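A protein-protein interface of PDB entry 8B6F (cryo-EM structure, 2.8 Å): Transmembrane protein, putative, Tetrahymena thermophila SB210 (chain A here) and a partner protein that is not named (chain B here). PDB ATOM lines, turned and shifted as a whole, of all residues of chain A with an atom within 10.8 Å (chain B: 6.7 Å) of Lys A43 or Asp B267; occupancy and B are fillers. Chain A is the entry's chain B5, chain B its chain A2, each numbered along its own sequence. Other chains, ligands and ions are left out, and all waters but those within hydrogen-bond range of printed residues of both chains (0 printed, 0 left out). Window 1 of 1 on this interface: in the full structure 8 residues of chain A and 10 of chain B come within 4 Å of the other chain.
NZ of Lys A43 lies within salt-bridge range of OD2 of Asp B267.
Hydrophobic or aromatic side chains of chain A within 4 Å of the printed part of chain B: Leu A35 and Met A36. Hydrophobic or aromatic side chains of chain B that line the printed part of chain A: Phe B260 and Met B264. Among the printed residues, 5 pairs touch across the chains.
Printed residues of chain B within 4 Å of Leu A35: Phe B260. Of the printed residues of chain B, Glu A39 touches Phe B260 and Met B264. Asn A40 touches none of the printed residues of chain B. Of chain B, only Asp B267 comes within 4 Å of Lys A43. Printed residues of chain A within 4 Å of Phe B260: Leu A35, Met A36 and Glu A39. Of chain A, only Glu A39 comes within 4 Å of Met B264. No residue of chain A comes within 4 Å of Leu B266. Of chain A, only Lys A43 comes within 4 Å of Asp B267. No residue of chain A comes within 4 Å of Leu B270. Gly B271 touches none of the printed residues of chain A. The nearest residue of chain B that does not touch Lys A43 is Met B264 (4.9 Å).
Among the printed residues, pairs that only touch across the chains: Met A36 with Phe B260 (3.5 Å), Leu A35 with Phe B260 (3.6 Å), Glu A39 with Phe B260 (3.8 Å) and Glu A39 with Met B264 (3.9 Å).
NZ of Lys A43 lies within salt-bridge range of OE2 of Glu A39.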
ATOM      1  N   PHE A  34      17.913  13.596 -17.978  1.00  0.00           N
ATOM      2  CA  PHE A  34      17.697  15.038 -18.041  1.00  0.00           C
ATOM      3  C   PHE A  34      18.894  15.744 -18.662  1.00  0.00           C
ATOM      4  O   PHE A  34      18.732  16.675 -19.459  1.00  0.00           O
ATOM      5  CB  PHE A  34      17.417  15.590 -16.644  1.00  0.00           C
ATOM      6  CG  PHE A  34      17.271  17.083 -16.605  1.00  0.00           C
ATOM      7  CD1 PHE A  34      16.052  17.680 -16.877  1.00  0.00           C
ATOM      8  CD2 PHE A  34      18.353  17.889 -16.296  1.00  0.00           C
ATOM      9  CE1 PHE A  34      15.915  19.056 -16.842  1.00  0.00           C
ATOM     10  CE2 PHE A  34      18.224  19.264 -16.260  1.00  0.00           C
ATOM     11  CZ  PHE A  34      17.004  19.849 -16.533  1.00  0.00           C
ATOM     12  N   LEU A  35      20.108  15.319 -18.304  1.00  0.00           N
ATOM     13  CA  LEU A  35      21.298  15.906 -18.910  1.00  0.00           C
ATOM     14  C   LEU A  35      21.317  15.665 -20.413  1.00  0.00           C
ATOM     15  O   LEU A  35      21.644  16.570 -21.190  1.00  0.00           O
ATOM     16  CB  LEU A  35      22.556  15.333 -18.258  1.00  0.00           C
ATOM     17  CG  LEU A  35      22.828  15.735 -16.804  1.00  0.00           C
ATOM     18  CD1 LEU A  35      24.105  15.081 -16.303  1.00  0.00           C
ATOM     19  CD2 LEU A  35      22.906  17.245 -16.636  1.00  0.00           C
ATOM     20  N   MET A  36      20.973  14.450 -20.844  1.00  0.00           N
ATOM     21  CA  MET A  36      20.926  14.163 -22.274  1.00  0.00           C
ATOM     22  C   MET A  36      19.938  15.083 -22.975  1.00  0.00           C
ATOM     23  O   MET A  36      20.254  15.690 -24.004  1.00  0.00           O
ATOM     24  CB  MET A  36      20.542  12.701 -22.501  1.00  0.00           C
ATOM     25  CG  MET A  36      21.635  11.705 -22.162  1.00  0.00           C
ATOM     26  SD  MET A  36      21.137  10.015 -22.537  1.00  0.00           S
ATOM     27  CE  MET A  36      22.593   9.109 -22.034  1.00  0.00           C
ATOM     28  N   PHE A  37      18.724  15.191 -22.432  1.00  0.00           N
ATOM     29  CA  PHE A  37      17.705  16.030 -23.050  1.00  0.00           C
ATOM     30  C   PHE A  37      18.161  17.482 -23.121  1.00  0.00           C
ATOM     31  O   PHE A  37      18.066  18.127 -24.169  1.00  0.00           O
ATOM     32  CB  PHE A  37      16.400  15.902 -22.263  1.00  0.00           C
ATOM     33  CG  PHE A  37      15.373  16.939 -22.606  1.00  0.00           C
ATOM     34  CD1 PHE A  37      14.522  16.760 -23.683  1.00  0.00           C
ATOM     35  CD2 PHE A  37      15.234  18.077 -21.830  1.00  0.00           C
ATOM     36  CE1 PHE A  37      13.567  17.707 -23.994  1.00  0.00           C
ATOM     37  CE2 PHE A  37      14.281  19.028 -22.134  1.00  0.00           C
ATOM     38  CZ  PHE A  37      13.446  18.842 -23.219  1.00  0.00           C
ATOM     39  N   TYR A  38      18.659  18.015 -22.003  1.00  0.00           N
ATOM     40  CA  TYR A  38      19.057  19.419 -21.969  1.00  0.00           C
ATOM     41  C   TYR A  38      20.231  19.689 -22.902  1.00  0.00           C
ATOM     42  O   TYR A  38      20.243  20.692 -23.623  1.00  0.00           O
ATOM     43  CB  TYR A  38      19.410  19.831 -20.541  1.00  0.00           C
ATOM     44  CG  TYR A  38      19.609  21.319 -20.381  1.00  0.00           C
ATOM     45  CD1 TYR A  38      20.836  21.910 -20.654  1.00  0.00           C
ATOM     46  CD2 TYR A  38      18.567  22.133 -19.965  1.00  0.00           C
ATOM     47  CE1 TYR A  38      21.018  23.270 -20.512  1.00  0.00           C
ATOM     48  CE2 TYR A  38      18.738  23.492 -19.820  1.00  0.00           C
ATOM     49  CZ  TYR A  38      19.965  24.057 -20.094  1.00  0.00           C
ATOM     50  OH  TYR A  38      20.136  25.412 -19.949  1.00  0.00           O
ATOM     51  N   GLU A  39      21.228  18.802 -22.903  1.00  0.00           N
ATOM     52  CA  GLU A  39      22.388  19.000 -23.764  1.00  0.00           C
ATOM     53  C   GLU A  39      22.001  18.922 -25.234  1.00  0.00           C
ATOM     54  O   GLU A  39      22.478  19.719 -26.049  1.00  0.00           O
ATOM     55  CB  GLU A  39      23.468  17.971 -23.431  1.00  0.00           C
ATOM     56  CG  GLU A  39      24.732  18.086 -24.275  1.00  0.00           C
ATOM     57  CD  GLU A  39      24.723  17.176 -25.490  1.00  0.00           C
ATOM     58  OE1 GLU A  39      23.639  16.689 -25.871  1.00  0.00           O
ATOM     59  OE2 GLU A  39      25.806  16.940 -26.064  1.00  0.00           O
ATOM     60  N   ASN A  40      21.141  17.968 -25.596  1.00  0.00           N
ATOM     61  CA  ASN A  40      20.690  17.877 -26.980  1.00  0.00           C
ATOM     62  C   ASN A  40      19.994  19.161 -27.413  1.00  0.00           C
ATOM     63  O   ASN A  40      20.318  19.733 -28.459  1.00  0.00           O
ATOM     64  CB  ASN A  40      19.758  16.676 -27.136  1.00  0.00           C
ATOM     65  CG  ASN A  40      19.219  16.536 -28.541  1.00  0.00           C
ATOM     66  OD1 ASN A  40      19.769  17.094 -29.488  1.00  0.00           O
ATOM     67  ND2 ASN A  40      18.135  15.784 -28.684  1.00  0.00           N
ATOM     68  N   ASN A  41      19.033  19.632 -26.616  1.00  0.00           N
ATOM     69  CA  ASN A  41      18.311  20.847 -26.975  1.00  0.00           C
ATOM     70  C   ASN A  41      19.242  22.052 -27.010  1.00  0.00           C
ATOM     71  O   ASN A  41      19.130  22.910 -27.892  1.00  0.00           O
ATOM     72  CB  ASN A  41      17.163  21.085 -25.997  1.00  0.00           C
ATOM     73  CG  ASN A  41      16.025  20.107 -26.192  1.00  0.00           C
ATOM     74  OD1 ASN A  41      16.155  19.124 -26.917  1.00  0.00           O
ATOM     75  ND2 ASN A  41      14.902  20.368 -25.536  1.00  0.00           N
ATOM     76  N   TYR A  42      20.171  22.134 -26.055  1.00  0.00           N
ATOM     77  CA  TYR A  42      21.087  23.268 -26.005  1.00  0.00           C
ATOM     78  C   TYR A  42      21.974  23.314 -27.242  1.00  0.00           C
ATOM     79  O   TYR A  42      22.159  24.374 -27.849  1.00  0.00           O
ATOM     80  CB  TYR A  42      21.936  23.187 -24.734  1.00  0.00           C
ATOM     81  CG  TYR A  42      22.887  24.346 -24.548  1.00  0.00           C
ATOM     82  CD1 TYR A  42      24.148  24.336 -25.128  1.00  0.00           C
ATOM     83  CD2 TYR A  42      22.531  25.440 -23.772  1.00  0.00           C
ATOM     84  CE1 TYR A  42      25.022  25.390 -24.952  1.00  0.00           C
ATOM     85  CE2 TYR A  42      23.397  26.498 -23.591  1.00  0.00           C
ATOM     86  CZ  TYR A  42      24.641  26.468 -24.184  1.00  0.00           C
ATOM     87  OH  TYR A  42      25.508  27.519 -24.006  1.00  0.00           O
ATOM     88  N   LYS A  43      22.527  22.167 -27.638  1.00  0.00           N
ATOM     89  CA  LYS A  43      23.386  22.142 -28.816  1.00  0.00           C
ATOM     90  C   LYS A  43      22.594  22.378 -30.093  1.00  0.00           C
ATOM     91  O   LYS A  43      23.124  22.947 -31.053  1.00  0.00           O
ATOM     92  CB  LYS A  43      24.139  20.814 -28.892  1.00  0.00           C
ATOM     93  CG  LYS A  43      25.265  20.696 -27.877  1.00  0.00           C
ATOM     94  CD  LYS A  43      26.011  19.386 -28.031  1.00  0.00           C
ATOM     95  CE  LYS A  43      27.220  19.327 -27.115  1.00  0.00           C
ATOM     96  NZ  LYS A  43      27.953  18.036 -27.242  1.00  0.00           N
ATOM     97  N   LYS A  44      21.332  21.947 -30.130  1.00  0.00           N
ATOM     98  CA  LYS A  44      20.494  22.201 -31.293  1.00  0.00           C
ATOM     99  C   LYS A  44      19.997  23.636 -31.348  1.00  0.00           C
ATOM    100  O   LYS A  44      19.610  24.101 -32.425  1.00  0.00           O
ATOM    101  CB  LYS A  44      19.298  21.246 -31.298  1.00  0.00           C
ATOM    102  CG  LYS A  44      18.444  21.326 -32.558  1.00  0.00           C
ATOM    103  CD  LYS A  44      17.314  20.304 -32.533  1.00  0.00           C
ATOM    104  CE  LYS A  44      16.491  20.367 -33.811  1.00  0.00           C
ATOM    105  NZ  LYS A  44      15.333  19.429 -33.784  1.00  0.00           N
ATOM    106  N   LEU A  45      20.001  24.347 -30.221  1.00  0.00           N
ATOM    107  CA  LEU A  45      19.432  25.685 -30.155  1.00  0.00           C
ATOM    108  C   LEU A  45      20.471  26.796 -30.177  1.00  0.00           C
ATOM    109  O   LEU A  45      20.157  27.904 -30.624  1.00  0.00           O
ATOM    110  CB  LEU A  45      18.577  25.822 -28.890  1.00  0.00           C
ATOM    111  CG  LEU A  45      17.792  27.122 -28.710  1.00  0.00           C
ATOM    112  CD1 LEU A  45      16.789  27.319 -29.834  1.00  0.00           C
ATOM    113  CD2 LEU A  45      17.089  27.120 -27.367  1.00  0.00           C
ATOM    114  N   TYR A  46      21.697  26.540 -29.714  1.00  0.00           N
ATOM    115  CA  TYR A  46      22.714  27.578 -29.612  1.00  0.00           C
ATOM    116  C   TYR A  46      23.994  27.284 -30.379  1.00  0.00           C
ATOM    117  O   TYR A  46      24.809  28.197 -30.549  1.00  0.00           O
ATOM    118  CB  TYR A  46      23.077  27.832 -28.140  1.00  0.00           C
ATOM    119  CG  TYR A  46      21.912  28.300 -27.305  1.00  0.00           C
ATOM    120  CD1 TYR A  46      21.315  29.529 -27.541  1.00  0.00           C
ATOM    121  CD2 TYR A  46      21.417  27.519 -26.273  1.00  0.00           C
ATOM    122  CE1 TYR A  46      20.252  29.962 -26.779  1.00  0.00           C
ATOM    123  CE2 TYR A  46      20.355  27.942 -25.504  1.00  0.00           C
ATOM    124  CZ  TYR A  46      19.776  29.164 -25.762  1.00  0.00           C
ATOM    125  OH  TYR A  46      18.717  29.591 -24.995  1.00  0.00           O
ATOM    126  N   LEU A  47      24.203  26.055 -30.837  1.00  0.00           N
ATOM    127  CA  LEU A  47      25.381  25.683 -31.611  1.00  0.00           C
ATOM    128  C   LEU A  47      24.979  25.178 -32.989  1.00  0.00           C
ATOM    129  O   LEU A  47      25.494  24.172 -33.480  1.00  0.00           O
ATOM    130  CB  LEU A  47      26.209  24.633 -30.874  1.00  0.00           C
ATOM    131  CG  LEU A  47      26.818  25.055 -29.535  1.00  0.00           C
ATOM    132  CD1 LEU A  47      27.643  23.920 -28.958  1.00  0.00           C
ATOM    133  CD2 LEU A  47      27.665  26.310 -29.673  1.00  0.00           C
ATOM    134  N   ASN A  48      24.047  25.877 -33.626  1.00  0.00           N
ATOM    135  CA  ASN A  48      23.550  25.519 -34.941  1.00  0.00           C
ATOM    136  C   ASN A  48      23.484  26.765 -35.810  1.00  0.00           C
ATOM    137  O   ASN A  48      23.236  27.862 -35.300  1.00  0.00           O
ATOM    138  CB  ASN A  48      22.157  24.878 -34.837  1.00  0.00           C
ATOM    139  CG  ASN A  48      21.684  24.287 -36.147  1.00  0.00           C
ATOM    140  OD1 ASN A  48      21.050  24.964 -36.955  1.00  0.00           O
ATOM    141  ND2 ASN A  48      21.986  23.013 -36.363  1.00  0.00           N
ATOM    142  N   PRO A  49      23.707  26.634 -37.121  1.00  0.00           N
ATOM    143  CA  PRO A  49      23.549  27.809 -37.994  1.00  0.00           C
ATOM    144  C   PRO A  49      22.157  28.408 -37.937  1.00  0.00           C
ATOM    145  O   PRO A  49      22.008  29.628 -38.082  1.00  0.00           O
ATOM    146  CB  PRO A  49      23.874  27.254 -39.389  1.00  0.00           C
ATOM    147  CG  PRO A  49      24.732  26.074 -39.135  1.00  0.00           C
ATOM    148  CD  PRO A  49      24.238  25.473 -37.856  1.00  0.00           C
ATOM    149  N   ARG A  50      21.131  27.584 -37.732  1.00  0.00           N
ATOM    150  CA  ARG A  50      19.756  28.052 -37.569  1.00  0.00           C
ATOM    151  C   ARG A  50      19.255  28.793 -38.805  1.00  0.00           C
ATOM    152  O   ARG A  50      18.426  29.700 -38.704  1.00  0.00           O
ATOM    153  CB  ARG A  50      19.621  28.936 -36.326  1.00  0.00           C
ATOM    154  CG  ARG A  50      19.853  28.181 -35.026  1.00  0.00           C
ATOM    155  CD  ARG A  50      19.759  29.091 -33.813  1.00  0.00           C
ATOM    156  NE  ARG A  50      18.439  29.692 -33.669  1.00  0.00           N
ATOM    157  CZ  ARG A  50      18.043  30.387 -32.612  1.00  0.00           C
ATOM    158  NH1 ARG A  50      18.839  30.577 -31.574  1.00  0.00           N
ATOM    159  NH2 ARG A  50      16.819  30.904 -32.595  1.00  0.00           N
ATOM    160  N   THR A  54      13.660  24.871 -37.648  1.00  0.00           N
ATOM    161  CA  THR A  54      13.571  23.560 -37.018  1.00  0.00           C
ATOM    162  C   THR A  54      12.875  23.578 -35.668  1.00  0.00           C
ATOM    163  O   THR A  54      12.211  22.599 -35.322  1.00  0.00           O
ATOM    164  CB  THR A  54      14.969  22.958 -36.840  1.00  0.00           C
ATOM    165  OG1 THR A  54      15.694  23.042 -38.073  1.00  0.00           O
ATOM    166  CG2 THR A  54      14.873  21.499 -36.420  1.00  0.00           C
ATOM    167  N   MET A  55      13.010  24.655 -34.895  1.00  0.00           N
ATOM    168  CA  MET A  55      12.365  24.755 -33.589  1.00  0.00           C
ATOM    169  C   MET A  55      11.301  25.843 -33.634  1.00  0.00           C
ATOM    170  O   MET A  55      11.629  27.036 -33.549  1.00  0.00           O
ATOM    171  CB  MET A  55      13.396  25.063 -32.499  1.00  0.00           C
ATOM    172  CG  MET A  55      14.417  23.960 -32.278  1.00  0.00           C
ATOM    173  SD  MET A  55      15.823  24.048 -33.397  1.00  0.00           S
ATOM    174  CE  MET A  55      16.676  25.477 -32.745  1.00  0.00           C
ATOM    175  N   LEU A  58      10.702  29.369 -31.260  1.00  0.00           N
ATOM    176  CA  LEU A  58      12.023  29.794 -30.816  1.00  0.00           C
ATOM    177  C   LEU A  58      12.812  30.485 -31.914  1.00  0.00           C
ATOM    178  O   LEU A  58      13.544  31.437 -31.634  1.00  0.00           O
ATOM    179  CB  LEU A  58      12.814  28.584 -30.300  1.00  0.00           C
ATOM    180  CG  LEU A  58      12.199  27.857 -29.102  1.00  0.00           C
ATOM    181  CD1 LEU A  58      13.025  26.641 -28.735  1.00  0.00           C
ATOM    182  CD2 LEU A  58      12.065  28.782 -27.905  1.00  0.00           C
ATOM    183  N   GLN A  59      12.683  30.030 -33.155  1.00  0.00           N
ATOM    184  CA  GLN A  59      13.244  30.737 -34.294  1.00  0.00           C
ATOM    185  C   GLN A  59      12.191  31.663 -34.888  1.00  0.00           C
ATOM    186  O   GLN A  59      10.995  31.361 -34.882  1.00  0.00           O
ATOM    187  CB  GLN A  59      13.730  29.756 -35.363  1.00  0.00           C
ATOM    188  CG  GLN A  59      14.806  28.796 -34.890  1.00  0.00           C
ATOM    189  CD  GLN A  59      15.427  28.021 -36.032  1.00  0.00           C
ATOM    190  OE1 GLN A  59      15.169  28.300 -37.200  1.00  0.00           O
ATOM    191  NE2 GLN A  59      16.254  27.038 -35.698  1.00  0.00           N
ATOM    192  N   PHE B 260      27.782   9.105 -23.193  1.00  0.00           N
ATOM    193  CA  PHE B 260      27.299  10.474 -23.329  1.00  0.00           C
ATOM    194  C   PHE B 260      28.013  11.416 -22.371  1.00  0.00           C
ATOM    195  O   PHE B 260      28.400  12.525 -22.756  1.00  0.00           O
ATOM    196  CB  PHE B 260      25.793  10.530 -23.085  1.00  0.00           C
ATOM    197  CG  PHE B 260      25.310  11.883 -22.658  1.00  0.00           C
ATOM    198  CD1 PHE B 260      25.089  12.882 -23.589  1.00  0.00           C
ATOM    199  CD2 PHE B 260      25.087  12.158 -21.320  1.00  0.00           C
ATOM    200  CE1 PHE B 260      24.652  14.129 -23.193  1.00  0.00           C
ATOM    201  CE2 PHE B 260      24.650  13.401 -20.918  1.00  0.00           C
ATOM    202  CZ  PHE B 260      24.431  14.387 -21.855  1.00  0.00           C
ATOM    203  N   TYR B 262      31.032  11.142 -21.004  1.00  0.00           N
ATOM    204  CA  TYR B 262      32.408  11.373 -21.419  1.00  0.00           C
ATOM    205  C   TYR B 262      32.465  12.256 -22.657  1.00  0.00           C
ATOM    206  O   TYR B 262      33.277  13.185 -22.731  1.00  0.00           O
ATOM    207  CB  TYR B 262      33.114  10.042 -21.665  1.00  0.00           C
ATOM    208  CG  TYR B 262      34.593  10.202 -21.893  1.00  0.00           C
ATOM    209  CD1 TYR B 262      35.457  10.428 -20.832  1.00  0.00           C
ATOM    210  CD2 TYR B 262      35.122  10.137 -23.170  1.00  0.00           C
ATOM    211  CE1 TYR B 262      36.812  10.582 -21.040  1.00  0.00           C
ATOM    212  CE2 TYR B 262      36.471  10.286 -23.387  1.00  0.00           C
ATOM    213  CZ  TYR B 262      37.312  10.510 -22.320  1.00  0.00           C
ATOM    214  OH  TYR B 262      38.659  10.661 -22.541  1.00  0.00           O
ATOM    215  N   ASN B 263      31.608  11.982 -23.643  1.00  0.00           N
ATOM    216  CA  ASN B 263      31.610  12.778 -24.866  1.00  0.00           C
ATOM    217  C   ASN B 263      31.193  14.215 -24.586  1.00  0.00           C
ATOM    218  O   ASN B 263      31.758  15.154 -25.157  1.00  0.00           O
ATOM    219  CB  ASN B 263      30.689  12.147 -25.907  1.00  0.00           C
ATOM    220  CG  ASN B 263      31.119  10.748 -26.296  1.00  0.00           C
ATOM    221  OD1 ASN B 263      32.307  10.432 -26.308  1.00  0.00           O
ATOM    222  ND2 ASN B 263      30.149   9.901 -26.624  1.00  0.00           N
ATOM    223  N   MET B 264      30.208  14.405 -23.707  1.00  0.00           N
ATOM    224  CA  MET B 264      29.787  15.754 -23.349  1.00  0.00           C
ATOM    225  C   MET B 264      30.909  16.511 -22.655  1.00  0.00           C
ATOM    226  O   MET B 264      31.126  17.698 -22.922  1.00  0.00           O
ATOM    227  CB  MET B 264      28.548  15.696 -22.457  1.00  0.00           C
ATOM    228  CG  MET B 264      28.027  17.060 -22.023  1.00  0.00           C
ATOM    229  SD  MET B 264      26.564  16.932 -20.977  1.00  0.00           S
ATOM    230  CE  MET B 264      26.171  18.659 -20.719  1.00  0.00           C
ATOM    231  N   GLU B 265      31.636  15.841 -21.760  1.00  0.00           N
ATOM    232  CA  GLU B 265      32.761  16.492 -21.102  1.00  0.00           C
ATOM    233  C   GLU B 265      33.837  16.878 -22.109  1.00  0.00           C
ATOM    234  O   GLU B 265      34.402  17.976 -22.035  1.00  0.00           O
ATOM    235  CB  GLU B 265      33.330  15.569 -20.025  1.00  0.00           C
ATOM    236  CG  GLU B 265      34.248  16.259 -19.037  1.00  0.00           C
ATOM    237  CD  GLU B 265      33.534  17.313 -18.217  1.00  0.00           C
ATOM    238  OE1 GLU B 265      32.288  17.369 -18.270  1.00  0.00           O
ATOM    239  OE2 GLU B 265      34.219  18.088 -17.519  1.00  0.00           O
ATOM    240  N   LEU B 266      34.140  15.988 -23.056  1.00  0.00           N
ATOM    241  CA  LEU B 266      35.123  16.318 -24.082  1.00  0.00           C
ATOM    242  C   LEU B 266      34.670  17.510 -24.913  1.00  0.00           C
ATOM    243  O   LEU B 266      35.459  18.420 -25.191  1.00  0.00           O
ATOM    244  CB  LEU B 266      35.377  15.117 -24.990  1.00  0.00           C
ATOM    245  CG  LEU B 266      36.148  13.930 -24.420  1.00  0.00           C
ATOM    246  CD1 LEU B 266      36.248  12.861 -25.491  1.00  0.00           C
ATOM    247  CD2 LEU B 266      37.526  14.331 -23.924  1.00  0.00           C
ATOM    248  N   ASP B 267      33.398  17.526 -25.312  1.00  0.00           N
ATOM    249  CA  ASP B 267      32.893  18.626 -26.125  1.00  0.00           C
ATOM    250  C   ASP B 267      32.929  19.935 -25.352  1.00  0.00           C
ATOM    251  O   ASP B 267      33.283  20.983 -25.905  1.00  0.00           O
ATOM    252  CB  ASP B 267      31.472  18.319 -26.594  1.00  0.00           C
ATOM    253  CG  ASP B 267      31.387  17.036 -27.397  1.00  0.00           C
ATOM    254  OD1 ASP B 267      32.433  16.379 -27.581  1.00  0.00           O
ATOM    255  OD2 ASP B 267      30.276  16.683 -27.845  1.00  0.00           O
ATOM    256  N   GLU B 268      32.563  19.898 -24.071  1.00  0.00           N
ATOM    257  CA  GLU B 268      32.643  21.100 -23.250  1.00  0.00           C
ATOM    258  C   GLU B 268      34.081  21.595 -23.149  1.00  0.00           C
ATOM    259  O   GLU B 268      34.337  22.802 -23.239  1.00  0.00           O
ATOM    260  CB  GLU B 268      32.072  20.819 -21.861  1.00  0.00           C
ATOM    261  CG  GLU B 268      32.023  22.031 -20.949  1.00  0.00           C
ATOM    262  CD  GLU B 268      31.554  21.681 -19.551  1.00  0.00           C
ATOM    263  OE1 GLU B 268      31.258  20.494 -19.305  1.00  0.00           O
ATOM    264  OE2 GLU B 268      31.484  22.590 -18.697  1.00  0.00           O
ATOM    265  N   GLY B 269      35.032  20.680 -22.956  1.00  0.00           N
ATOM    266  CA  GLY B 269      36.428  21.084 -22.896  1.00  0.00           C
ATOM    267  C   GLY B 269      36.919  21.695 -24.195  1.00  0.00           C
ATOM    268  O   GLY B 269      37.620  22.708 -24.189  1.00  0.00           O
ATOM    269  N   LEU B 270      36.558  21.086 -25.326  1.00  0.00           N
ATOM    270  CA  LEU B 270      36.980  21.620 -26.616  1.00  0.00           C
ATOM    271  C   LEU B 270      36.379  22.996 -26.861  1.00  0.00           C
ATOM    272  O   LEU B 270      37.062  23.904 -27.348  1.00  0.00           O
ATOM    273  CB  LEU B 270      36.595  20.656 -27.736  1.00  0.00           C
ATOM    274  CG  LEU B 270      37.299  19.297 -27.711  1.00  0.00           C
ATOM    275  CD1 LEU B 270      36.695  18.368 -28.748  1.00  0.00           C
ATOM    276  CD2 LEU B 270      38.794  19.453 -27.941  1.00  0.00           C
ATOM    277  N   GLY B 271      35.096  23.166 -26.543  1.00  0.00           N
ATOM    278  CA  GLY B 271      34.481  24.474 -26.687  1.00  0.00           C
ATOM    279  C   GLY B 271      35.114  25.511 -25.780  1.00  0.00           C
ATOM    280  O   GLY B 271      35.343  26.651 -26.189  1.00  0.00           O
ATOM    281  N   GLY B 272      35.419  25.126 -24.541  1.00  0.00           N
ATOM    282  CA  GLY B 272      36.093  26.045 -23.640  1.00  0.00           C
ATOM    283  C   GLY B 272      37.455  26.465 -24.158  1.00  0.00           C
ATOM    284  O   GLY B 272      37.817  27.642 -24.100  1.00  0.00           O
